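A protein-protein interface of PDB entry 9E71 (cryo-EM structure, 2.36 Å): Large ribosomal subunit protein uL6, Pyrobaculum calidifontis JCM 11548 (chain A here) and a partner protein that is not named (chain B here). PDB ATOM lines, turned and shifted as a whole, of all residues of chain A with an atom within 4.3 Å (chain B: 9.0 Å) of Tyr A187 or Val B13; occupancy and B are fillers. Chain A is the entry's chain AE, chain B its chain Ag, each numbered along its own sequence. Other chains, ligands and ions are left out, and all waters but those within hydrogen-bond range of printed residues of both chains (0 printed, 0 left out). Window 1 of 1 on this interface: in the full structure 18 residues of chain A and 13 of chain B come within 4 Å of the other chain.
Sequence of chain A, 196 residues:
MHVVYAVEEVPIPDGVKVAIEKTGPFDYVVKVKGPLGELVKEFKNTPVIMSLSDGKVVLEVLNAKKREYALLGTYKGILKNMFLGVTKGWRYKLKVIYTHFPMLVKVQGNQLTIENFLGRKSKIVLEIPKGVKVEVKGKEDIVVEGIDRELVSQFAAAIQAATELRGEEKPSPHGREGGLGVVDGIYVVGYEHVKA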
ATOM      1  N   LEU A  94      17.214  -3.801  -2.676  1.00  0.00           N
ATOM      2  CA  LEU A  94      17.145  -2.357  -2.546  1.00  0.00           C
ATOM      3  C   LEU A  94      17.399  -1.983  -1.097  1.00  0.00           C
ATOM      4  O   LEU A  94      17.017  -2.716  -0.185  1.00  0.00           O
ATOM      5  CB  LEU A  94      15.784  -1.818  -3.000  1.00  0.00           C
ATOM      6  CG  LEU A  94      15.380  -2.135  -4.440  1.00  0.00           C
ATOM      7  CD1 LEU A  94      14.612  -3.437  -4.506  1.00  0.00           C
ATOM      8  CD2 LEU A  94      14.559  -1.007  -5.027  1.00  0.00           C
ATOM      9  N   LYS A  95      18.036  -0.838  -0.894  1.00  0.00           N
ATOM     10  CA  LYS A  95      18.372  -0.347   0.432  1.00  0.00           C
ATOM     11  C   LYS A  95      17.554   0.899   0.737  1.00  0.00           C
ATOM     12  O   LYS A  95      17.279   1.708  -0.154  1.00  0.00           O
ATOM     13  CB  LYS A  95      19.861  -0.030   0.537  1.00  0.00           C
ATOM     14  CG  LYS A  95      20.384   0.022   1.956  1.00  0.00           C
ATOM     15  CD  LYS A  95      20.780  -1.363   2.437  1.00  0.00           C
ATOM     16  CE  LYS A  95      22.132  -1.345   3.137  1.00  0.00           C
ATOM     17  NZ  LYS A  95      22.189  -0.339   4.234  1.00  0.00           N
ATOM     18  N   ILE A  97      17.479   4.324   2.742  1.00  0.00           N
ATOM     19  CA  ILE A  97      18.419   5.280   3.310  1.00  0.00           C
ATOM     20  C   ILE A  97      17.624   6.475   3.800  1.00  0.00           C
ATOM     21  O   ILE A  97      16.871   7.082   3.029  1.00  0.00           O
ATOM     22  CB  ILE A  97      19.486   5.705   2.290  1.00  0.00           C
ATOM     23  CG1 ILE A  97      20.367   4.507   1.932  1.00  0.00           C
ATOM     24  CG2 ILE A  97      20.313   6.862   2.835  1.00  0.00           C
ATOM     25  CD1 ILE A  97      21.411   4.790   0.876  1.00  0.00           C
ATOM     26  N   GLN A 160      12.906   2.748  -6.724  1.00  0.00           N
ATOM     27  CA  GLN A 160      13.955   3.744  -6.524  1.00  0.00           C
ATOM     28  C   GLN A 160      13.487   5.130  -6.953  1.00  0.00           C
ATOM     29  O   GLN A 160      13.722   6.121  -6.253  1.00  0.00           O
ATOM     30  CB  GLN A 160      15.214   3.344  -7.286  1.00  0.00           C
ATOM     31  CG  GLN A 160      16.142   4.507  -7.568  1.00  0.00           C
ATOM     32  CD  GLN A 160      17.599   4.143  -7.396  1.00  0.00           C
ATOM     33  OE1 GLN A 160      17.989   2.993  -7.589  1.00  0.00           O
ATOM     34  NE2 GLN A 160      18.414   5.122  -7.033  1.00  0.00           N
ATOM     35  N   VAL A 183      19.798  13.290   1.378  1.00  0.00           N
ATOM     36  CA  VAL A 183      19.808  12.160   0.453  1.00  0.00           C
ATOM     37  C   VAL A 183      19.031  11.041   1.133  1.00  0.00           C
ATOM     38  O   VAL A 183      19.577  10.229   1.884  1.00  0.00           O
ATOM     39  CB  VAL A 183      21.225  11.722   0.071  1.00  0.00           C
ATOM     40  CG1 VAL A 183      21.804  12.673  -0.969  1.00  0.00           C
ATOM     41  CG2 VAL A 183      22.120  11.680   1.298  1.00  0.00           C
ATOM     42  N   ASP A 184      17.736  10.993   0.865  1.00  0.00           N
ATOM     43  CA  ASP A 184      16.830  10.060   1.508  1.00  0.00           C
ATOM     44  C   ASP A 184      16.105   9.280   0.424  1.00  0.00           C
ATOM     45  O   ASP A 184      15.610   9.866  -0.544  1.00  0.00           O
ATOM     46  CB  ASP A 184      15.828  10.819   2.369  1.00  0.00           C
ATOM     47  CG  ASP A 184      16.385  11.194   3.717  1.00  0.00           C
ATOM     48  OD1 ASP A 184      17.134  12.188   3.785  1.00  0.00           O
ATOM     49  OD2 ASP A 184      16.030  10.557   4.716  1.00  0.00           O
ATOM     50  N   GLY A 185      16.061   7.962   0.560  1.00  0.00           N
ATOM     51  CA  GLY A 185      15.271   7.188  -0.371  1.00  0.00           C
ATOM     52  C   GLY A 185      15.677   5.731  -0.386  1.00  0.00           C
ATOM     53  O   GLY A 185      16.342   5.234   0.522  1.00  0.00           O
ATOM     54  N   ILE A 186      15.240   5.061  -1.445  1.00  0.00           N
ATOM     55  CA  ILE A 186      15.463   3.639  -1.648  1.00  0.00           C
ATOM     56  C   ILE A 186      16.317   3.480  -2.892  1.00  0.00           C
ATOM     57  O   ILE A 186      15.950   3.963  -3.970  1.00  0.00           O
ATOM     58  CB  ILE A 186      14.142   2.873  -1.783  1.00  0.00           C
ATOM     59  CG1 ILE A 186      13.278   3.093  -0.541  1.00  0.00           C
ATOM     60  CG2 ILE A 186      14.412   1.409  -2.012  1.00  0.00           C
ATOM     61  CD1 ILE A 186      11.901   2.500  -0.647  1.00  0.00           C
ATOM     62  N   TYR A 187      17.446   2.800  -2.745  1.00  0.00           N
ATOM     63  CA  TYR A 187      18.445   2.688  -3.798  1.00  0.00           C
ATOM     64  C   TYR A 187      18.598   1.226  -4.181  1.00  0.00           C
ATOM     65  O   TYR A 187      18.804   0.374  -3.313  1.00  0.00           O
ATOM     66  CB  TYR A 187      19.785   3.266  -3.346  1.00  0.00           C
ATOM     67  CG  TYR A 187      19.740   4.734  -2.989  1.00  0.00           C
ATOM     68  CD1 TYR A 187      19.315   5.158  -1.740  1.00  0.00           C
ATOM     69  CD2 TYR A 187      20.117   5.698  -3.909  1.00  0.00           C
ATOM     70  CE1 TYR A 187      19.272   6.492  -1.418  1.00  0.00           C
ATOM     71  CE2 TYR A 187      20.076   7.037  -3.596  1.00  0.00           C
ATOM     72  CZ  TYR A 187      19.653   7.428  -2.348  1.00  0.00           C
ATOM     73  OH  TYR A 187      19.609   8.761  -2.024  1.00  0.00           O
ATOM     74  N   VAL A 188      18.495   0.939  -5.478  1.00  0.00           N
ATOM     75  CA  VAL A 188      18.761  -0.409  -5.960  1.00  0.00           C
ATOM     76  C   VAL A 188      20.237  -0.703  -5.760  1.00  0.00           C
ATOM     77  O   VAL A 188      21.103  -0.009  -6.304  1.00  0.00           O
ATOM     78  CB  VAL A 188      18.358  -0.554  -7.429  1.00  0.00           C
ATOM     79  CG1 VAL A 188      18.542  -1.985  -7.881  1.00  0.00           C
ATOM     80  CG2 VAL A 188      16.920  -0.111  -7.633  1.00  0.00           C
ATOM     81  N   VAL A 189      20.533  -1.736  -4.975  1.00  0.00           N
ATOM     82  CA  VAL A 189      21.907  -2.051  -4.596  1.00  0.00           C
ATOM     83  C   VAL A 189      22.518  -3.144  -5.449  1.00  0.00           C
ATOM     84  O   VAL A 189      23.753  -3.278  -5.460  1.00  0.00           O
ATOM     85  CB  VAL A 189      22.003  -2.441  -3.107  1.00  0.00           C
ATOM     86  CG1 VAL A 189      21.589  -1.281  -2.241  1.00  0.00           C
ATOM     87  CG2 VAL A 189      21.139  -3.651  -2.823  1.00  0.00           C
ATOM     88  N   ILE B   3      24.083  15.696   8.891  1.00  0.00           N
ATOM     89  CA  ILE B   3      23.741  14.685   7.900  1.00  0.00           C
ATOM     90  C   ILE B   3      24.956  13.823   7.601  1.00  0.00           C
ATOM     91  O   ILE B   3      25.863  14.243   6.885  1.00  0.00           O
ATOM     92  CB  ILE B   3      23.191  15.326   6.617  1.00  0.00           C
ATOM     93  CG1 ILE B   3      21.905  16.097   6.919  1.00  0.00           C
ATOM     94  CG2 ILE B   3      22.951  14.267   5.554  1.00  0.00           C
ATOM     95  CD1 ILE B   3      21.118  16.482   5.686  1.00  0.00           C
ATOM     96  N   LEU B   5      26.214   9.466   7.127  1.00  0.00           N
ATOM     97  CA  LEU B   5      25.830   8.077   6.930  1.00  0.00           C
ATOM     98  C   LEU B   5      27.043   7.176   7.093  1.00  0.00           C
ATOM     99  O   LEU B   5      28.181   7.613   6.904  1.00  0.00           O
ATOM    100  CB  LEU B   5      25.216   7.866   5.545  1.00  0.00           C
ATOM    101  CG  LEU B   5      23.839   8.487   5.320  1.00  0.00           C
ATOM    102  CD1 LEU B   5      23.518   8.565   3.835  1.00  0.00           C
ATOM    103  CD2 LEU B   5      22.771   7.705   6.065  1.00  0.00           C
ATOM    104  N   ASP B   6      26.791   5.913   7.431  1.00  0.00           N
ATOM    105  CA  ASP B   6      27.854   4.930   7.532  1.00  0.00           C
ATOM    106  C   ASP B   6      28.463   4.689   6.154  1.00  0.00           C
ATOM    107  O   ASP B   6      27.855   5.034   5.141  1.00  0.00           O
ATOM    108  CB  ASP B   6      27.319   3.628   8.114  1.00  0.00           C
ATOM    109  CG  ASP B   6      26.071   3.157   7.417  1.00  0.00           C
ATOM    110  OD1 ASP B   6      25.541   3.925   6.594  1.00  0.00           O
ATOM    111  OD2 ASP B   6      25.623   2.024   7.684  1.00  0.00           O
ATOM    112  N   PRO B   7      29.680   4.125   6.102  1.00  0.00           N
ATOM    113  CA  PRO B   7      30.432   4.063   4.831  1.00  0.00           C
ATOM    114  C   PRO B   7      29.745   3.328   3.689  1.00  0.00           C
ATOM    115  O   PRO B   7      29.877   3.747   2.534  1.00  0.00           O
ATOM    116  CB  PRO B   7      31.729   3.355   5.242  1.00  0.00           C
ATOM    117  CG  PRO B   7      31.888   3.668   6.674  1.00  0.00           C
ATOM    118  CD  PRO B   7      30.509   3.730   7.252  1.00  0.00           C
ATOM    119  N   GLU B   8      28.996   2.263   3.974  1.00  0.00           N
ATOM    120  CA  GLU B   8      28.305   1.546   2.907  1.00  0.00           C
ATOM    121  C   GLU B   8      27.197   2.396   2.294  1.00  0.00           C
ATOM    122  O   GLU B   8      27.088   2.508   1.066  1.00  0.00           O
ATOM    123  CB  GLU B   8      27.741   0.235   3.444  1.00  0.00           C
ATOM    124  CG  GLU B   8      26.925  -0.542   2.437  1.00  0.00           C
ATOM    125  CD  GLU B   8      25.610  -1.012   3.013  1.00  0.00           C
ATOM    126  OE1 GLU B   8      25.158  -0.424   4.016  1.00  0.00           O
ATOM    127  OE2 GLU B   8      25.031  -1.973   2.465  1.00  0.00           O
ATOM    128  N   LYS B   9      26.367   3.007   3.140  1.00  0.00           N
ATOM    129  CA  LYS B   9      25.317   3.885   2.642  1.00  0.00           C
ATOM    130  C   LYS B   9      25.910   5.107   1.960  1.00  0.00           C
ATOM    131  O   LYS B   9      25.350   5.616   0.983  1.00  0.00           O
ATOM    132  CB  LYS B   9      24.399   4.298   3.788  1.00  0.00           C
ATOM    133  CG  LYS B   9      23.607   3.150   4.381  1.00  0.00           C
ATOM    134  CD  LYS B   9      22.737   3.618   5.533  1.00  0.00           C
ATOM    135  CE  LYS B   9      22.021   2.456   6.192  1.00  0.00           C
ATOM    136  NZ  LYS B   9      21.245   2.894   7.379  1.00  0.00           N
ATOM    137  N   LEU B  10      27.046   5.590   2.464  1.00  0.00           N
ATOM    138  CA  LEU B  10      27.720   6.726   1.850  1.00  0.00           C
ATOM    139  C   LEU B  10      28.184   6.381   0.444  1.00  0.00           C
ATOM    140  O   LEU B  10      27.998   7.166  -0.492  1.00  0.00           O
ATOM    141  CB  LEU B  10      28.900   7.161   2.720  1.00  0.00           C
ATOM    142  CG  LEU B  10      29.999   8.030   2.102  1.00  0.00           C
ATOM    143  CD1 LEU B  10      29.433   9.268   1.411  1.00  0.00           C
ATOM    144  CD2 LEU B  10      31.007   8.423   3.160  1.00  0.00           C
ATOM    145  N   ALA B  11      28.779   5.197   0.275  1.00  0.00           N
ATOM    146  CA  ALA B  11      29.200   4.758  -1.050  1.00  0.00           C
ATOM    147  C   ALA B  11      28.006   4.576  -1.977  1.00  0.00           C
ATOM    148  O   ALA B  11      28.071   4.926  -3.160  1.00  0.00           O
ATOM    149  CB  ALA B  11      29.997   3.460  -0.943  1.00  0.00           C
ATOM    150  N   ILE B  12      26.903   4.041  -1.449  1.00  0.00           N
ATOM    151  CA  ILE B  12      25.699   3.827  -2.252  1.00  0.00           C
ATOM    152  C   ILE B  12      25.139   5.157  -2.744  1.00  0.00           C
ATOM    153  O   ILE B  12      24.809   5.320  -3.926  1.00  0.00           O
ATOM    154  CB  ILE B  12      24.657   3.056  -1.427  1.00  0.00           C
ATOM    155  CG1 ILE B  12      25.014   1.577  -1.376  1.00  0.00           C
ATOM    156  CG2 ILE B  12      23.276   3.243  -2.011  1.00  0.00           C
ATOM    157  CD1 ILE B  12      23.868   0.715  -0.979  1.00  0.00           C
ATOM    158  N   VAL B  13      25.040   6.132  -1.842  1.00  0.00           N
ATOM    159  CA  VAL B  13      24.491   7.434  -2.198  1.00  0.00           C
ATOM    160  C   VAL B  13      25.426   8.170  -3.146  1.00  0.00           C
ATOM    161  O   VAL B  13      24.975   8.864  -4.063  1.00  0.00           O
ATOM    162  CB  VAL B  13      24.213   8.255  -0.926  1.00  0.00           C
ATOM    163  CG1 VAL B  13      24.316   9.738  -1.218  1.00  0.00           C
ATOM    164  CG2 VAL B  13      22.848   7.910  -0.370  1.00  0.00           C
ATOM    165  N   LEU B  14      26.739   8.040  -2.940  1.00  0.00           N
ATOM    166  CA  LEU B  14      27.695   8.675  -3.839  1.00  0.00           C
ATOM    167  C   LEU B  14      27.614   8.077  -5.235  1.00  0.00           C
ATOM    168  O   LEU B  14      27.719   8.796  -6.235  1.00  0.00           O
ATOM    169  CB  LEU B  14      29.108   8.541  -3.277  1.00  0.00           C
ATOM    170  CG  LEU B  14      29.656   9.771  -2.553  1.00  0.00           C
ATOM    171  CD1 LEU B  14      30.190  10.782  -3.543  1.00  0.00           C
ATOM    172  CD2 LEU B  14      28.574  10.395  -1.698  1.00  0.00           C
ATOM    173  N   GLN B  15      27.426   6.761  -5.322  1.00  0.00           N
ATOM    174  CA  GLN B  15      27.286   6.122  -6.620  1.00  0.00           C
ATOM    175  C   GLN B  15      25.981   6.508  -7.304  1.00  0.00           C
ATOM    176  O   GLN B  15      25.950   6.660  -8.528  1.00  0.00           O
ATOM    177  CB  GLN B  15      27.372   4.608  -6.463  1.00  0.00           C
ATOM    178  CG  GLN B  15      26.601   3.843  -7.507  1.00  0.00           C
ATOM    179  CD  GLN B  15      27.468   3.435  -8.674  1.00  0.00           C
ATOM    180  OE1 GLN B  15      28.580   3.933  -8.837  1.00  0.00           O
ATOM    181  NE2 GLN B  15      26.965   2.525  -9.495  1.00  0.00           N
ATOM    182  N   HIS B  16      24.899   6.666  -6.545  1.00  0.00           N
ATOM    183  CA  HIS B  16      23.603   6.897  -7.170  1.00  0.00           C
ATOM    184  C   HIS B  16      23.276   8.368  -7.386  1.00  0.00           C
ATOM    185  O   HIS B  16      22.371   8.678  -8.166  1.00  0.00           O
ATOM    186  CB  HIS B  16      22.496   6.254  -6.336  1.00  0.00           C
ATOM    187  CG  HIS B  16      22.259   4.816  -6.664  1.00  0.00           C
ATOM    188  ND1 HIS B  16      21.333   4.412  -7.600  1.00  0.00           N
ATOM    189  CD2 HIS B  16      22.832   3.688  -6.188  1.00  0.00           C
ATOM    190  CE1 HIS B  16      21.345   3.095  -7.684  1.00  0.00           C
ATOM    191  NE2 HIS B  16      22.245   2.630  -6.837  1.00  0.00           N
ATOM    192  N   ARG B  17      23.988   9.283  -6.732  1.00  0.00           N
ATOM    193  CA  ARG B  17      23.647  10.694  -6.788  1.00  0.00           C
ATOM    194  C   ARG B  17      24.780  11.600  -7.244  1.00  0.00           C
ATOM    195  O   ARG B  17      24.512  12.750  -7.608  1.00  0.00           O
ATOM    196  CB  ARG B  17      23.161  11.180  -5.414  1.00  0.00           C
ATOM    197  CG  ARG B  17      21.900  10.504  -4.926  1.00  0.00           C
ATOM    198  CD  ARG B  17      20.803  11.517  -4.676  1.00  0.00           C
ATOM    199  NE  ARG B  17      19.674  10.930  -3.965  1.00  0.00           N
ATOM    200  CZ  ARG B  17      18.408  11.044  -4.344  1.00  0.00           C
ATOM    201  NH1 ARG B  17      18.069  11.735  -5.418  1.00  0.00           N
ATOM    202  NH2 ARG B  17      17.459  10.448  -3.627  1.00  0.00           N
ATOM    203  N   PHE B  18      26.028  11.130  -7.236  1.00  0.00           N
ATOM    204  CA  PHE B  18      27.165  11.994  -7.523  1.00  0.00           C
ATOM    205  C   PHE B  18      28.149  11.332  -8.477  1.00  0.00           C
ATOM    206  O   PHE B  18      29.356  11.589  -8.400  1.00  0.00           O
ATOM    207  CB  PHE B  18      27.905  12.381  -6.241  1.00  0.00           C
ATOM    208  CG  PHE B  18      27.061  13.105  -5.235  1.00  0.00           C
ATOM    209  CD1 PHE B  18      26.298  12.407  -4.315  1.00  0.00           C
ATOM    210  CD2 PHE B  18      27.056  14.485  -5.186  1.00  0.00           C
ATOM    211  CE1 PHE B  18      25.534  13.070  -3.389  1.00  0.00           C
ATOM    212  CE2 PHE B  18      26.293  15.154  -4.256  1.00  0.00           C
ATOM    213  CZ  PHE B  18      25.532  14.446  -3.357  1.00  0.00           C
ATOM    214  N   ASN B  19      27.670  10.475  -9.371  1.00  0.00           N
ATOM    215  CA  ASN B  19      28.548   9.647 -10.190  1.00  0.00           C
ATOM    216  C   ASN B  19      28.177   9.745 -11.658  1.00  0.00           C
ATOM    217  O   ASN B  19      28.006   8.738 -12.348  1.00  0.00           O
ATOM    218  CB  ASN B  19      28.515   8.192  -9.742  1.00  0.00           C
ATOM    219  CG  ASN B  19      29.719   7.415 -10.225  1.00  0.00           C
ATOM    220  OD1 ASN B  19      30.764   7.993 -10.512  1.00  0.00           O
ATOM    221  ND2 ASN B  19      29.575   6.102 -10.331  1.00  0.00           N
ATOM    222  N   TYR B  20      28.039  10.959 -12.172  1.00  0.00           N
ATOM    223  CA  TYR B  20      27.704  11.106 -13.576  1.00  0.00           C
ATOM    224  C   TYR B  20      28.247  12.429 -14.095  1.00  0.00           C
ATOM    225  O   TYR B  20      28.922  13.179 -13.383  1.00  0.00           O
ATOM    226  CB  TYR B  20      26.192  10.987 -13.790  1.00  0.00           C
ATOM    227  CG  TYR B  20      25.360  11.925 -12.948  1.00  0.00           C
ATOM    228  CD1 TYR B  20      24.938  11.565 -11.675  1.00  0.00           C
ATOM    229  CD2 TYR B  20      24.986  13.165 -13.433  1.00  0.00           C
ATOM    230  CE1 TYR B  20      24.175  12.421 -10.911  1.00  0.00           C
ATOM    231  CE2 TYR B  20      24.223  14.022 -12.680  1.00  0.00           C
ATOM    232  CZ  TYR B  20      23.819  13.646 -11.421  1.00  0.00           C
ATOM    233  OH  TYR B  20      23.060  14.513 -10.673  1.00  0.00           O
ATOM    234  N   LYS B  48      30.059  15.691 -12.328  1.00  0.00           N
ATOM    235  CA  LYS B  48      29.618  16.178 -11.030  1.00  0.00           C
ATOM    236  C   LYS B  48      30.574  15.698  -9.949  1.00  0.00           C
ATOM    237  O   LYS B  48      30.946  14.522  -9.914  1.00  0.00           O
ATOM    238  CB  LYS B  48      28.196  15.713 -10.728  1.00  0.00           C
ATOM    239  CG  LYS B  48      27.144  16.718 -11.135  1.00  0.00           C
ATOM    240  CD  LYS B  48      25.775  16.273 -10.690  1.00  0.00           C
ATOM    241  CE  LYS B  48      25.843  15.528  -9.375  1.00  0.00           C
ATOM    242  NZ  LYS B  48      25.918  16.462  -8.224  1.00  0.00           N
ATOM    243  N   PHE B  50      31.482  15.446  -5.828  1.00  0.00           N
ATOM    244  CA  PHE B  50      31.066  15.524  -4.438  1.00  0.00           C
ATOM    245  C   PHE B  50      32.187  16.156  -3.624  1.00  0.00           C
ATOM    246  O   PHE B  50      33.325  15.677  -3.645  1.00  0.00           O
ATOM    247  CB  PHE B  50      30.721  14.140  -3.891  1.00  0.00           C
ATOM    248  CG  PHE B  50      30.619  14.092  -2.398  1.00  0.00           C
ATOM    249  CD1 PHE B  50      29.555  14.686  -1.748  1.00  0.00           C
ATOM    250  CD2 PHE B  50      31.589  13.458  -1.643  1.00  0.00           C
ATOM    251  CE1 PHE B  50      29.458  14.647  -0.375  1.00  0.00           C
ATOM    252  CE2 PHE B  50      31.495  13.416  -0.271  1.00  0.00           C
ATOM    253  CZ  PHE B  50      30.429  14.013   0.363  1.00  0.00           C
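The side-chain amino group (NZ) of Lys A95 lies within salt-bridge range of the side-chain carboxylate (OE1) of Glu B8, at 3.0 Å.
NE2 of Gln A160 lies within hydrogen-bond range of ND1 of His B16 (3.1 Å).
The backbone carbonyl oxygen (O) of Val A188 lies within hydrogen-bond range of a ring nitrogen (NE2) of His B16, at 2.9 Å.
The side-chain hydroxyl (OH) of Tyr A187 lies within hydrogen-bond range of the guanidinium group (NE) of Arg B17 (2.9 Å).
The backbone carbonyl oxygen (O) of Tyr A187 lies within hydrogen-bond range of the backbone NH (N) of Lys A95, 2.8 Å away.
The backbone carbonyl oxygen (O) of Gly A185 is in hydrogen-bond range of the backbone NH (N) of Ile A97, at 2.7 Å.
The side-chain amide oxygen (OE1) of Gln A160 is in hydrogen-bond range of the backbone NH (N) of Val A188 (3.0 Å).
Lys A95 touches Lys B9 (NZ to CE, 3.4 Å).
Ile A97 touches Leu B5.
CG2 of Ile B12 touches CD1 of Ile A97, at 3.8 Å.
Ile A97 touches Val B13 (CD1 to CG2, 3.7 Å).
CG2 of Val A183 touches CG1 of Val B13, at 3.9 Å.
O of Asp A184 touches NH2 of Arg B17, 3.6 Å away.
Ile B12 touches Tyr A187 (CG2 to CB, 3.7 Å).
Val B13 touches Tyr A187 (CG2 to OH, 3.7 Å).
Tyr A187 touches His B16.
CG1 of Val A189 touches CD1 of Ile B12 (3.3 Å).
No residue of chain B comes within 4 Å of Gly A185.
Tyr A187 touches just these residues of chain B: Ile B12, Val B13, His B16 and Arg B17.
Printed residues of chain A within 4 Å of Leu B5: Ile A97.
Of the printed residues of chain A, Ile B12 touches Ile A97, Tyr A187 and Val A189.
Of chain A, only Ile A97 (3.7 Å), Val A183 (3.9 Å) and Tyr A187 (3.7 Å) come within 4 Å of Val B13.
Of the printed residues of chain A, His B16 touches Gln A160, Tyr A187 and Val A188.
Of the 19 printed residues of chain B, 7 touch a printed residue of chain A.
Hydrophobic or aromatic side chains of chain B within 4 Å of the printed part of chain A: Leu B5, Ile B12, Val B13 and His B16.
Along chain A the printed residues that touch a printed residue of chain B span positions 95 to 189.
Among the printed residues, 14 pairs touch across the chains.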
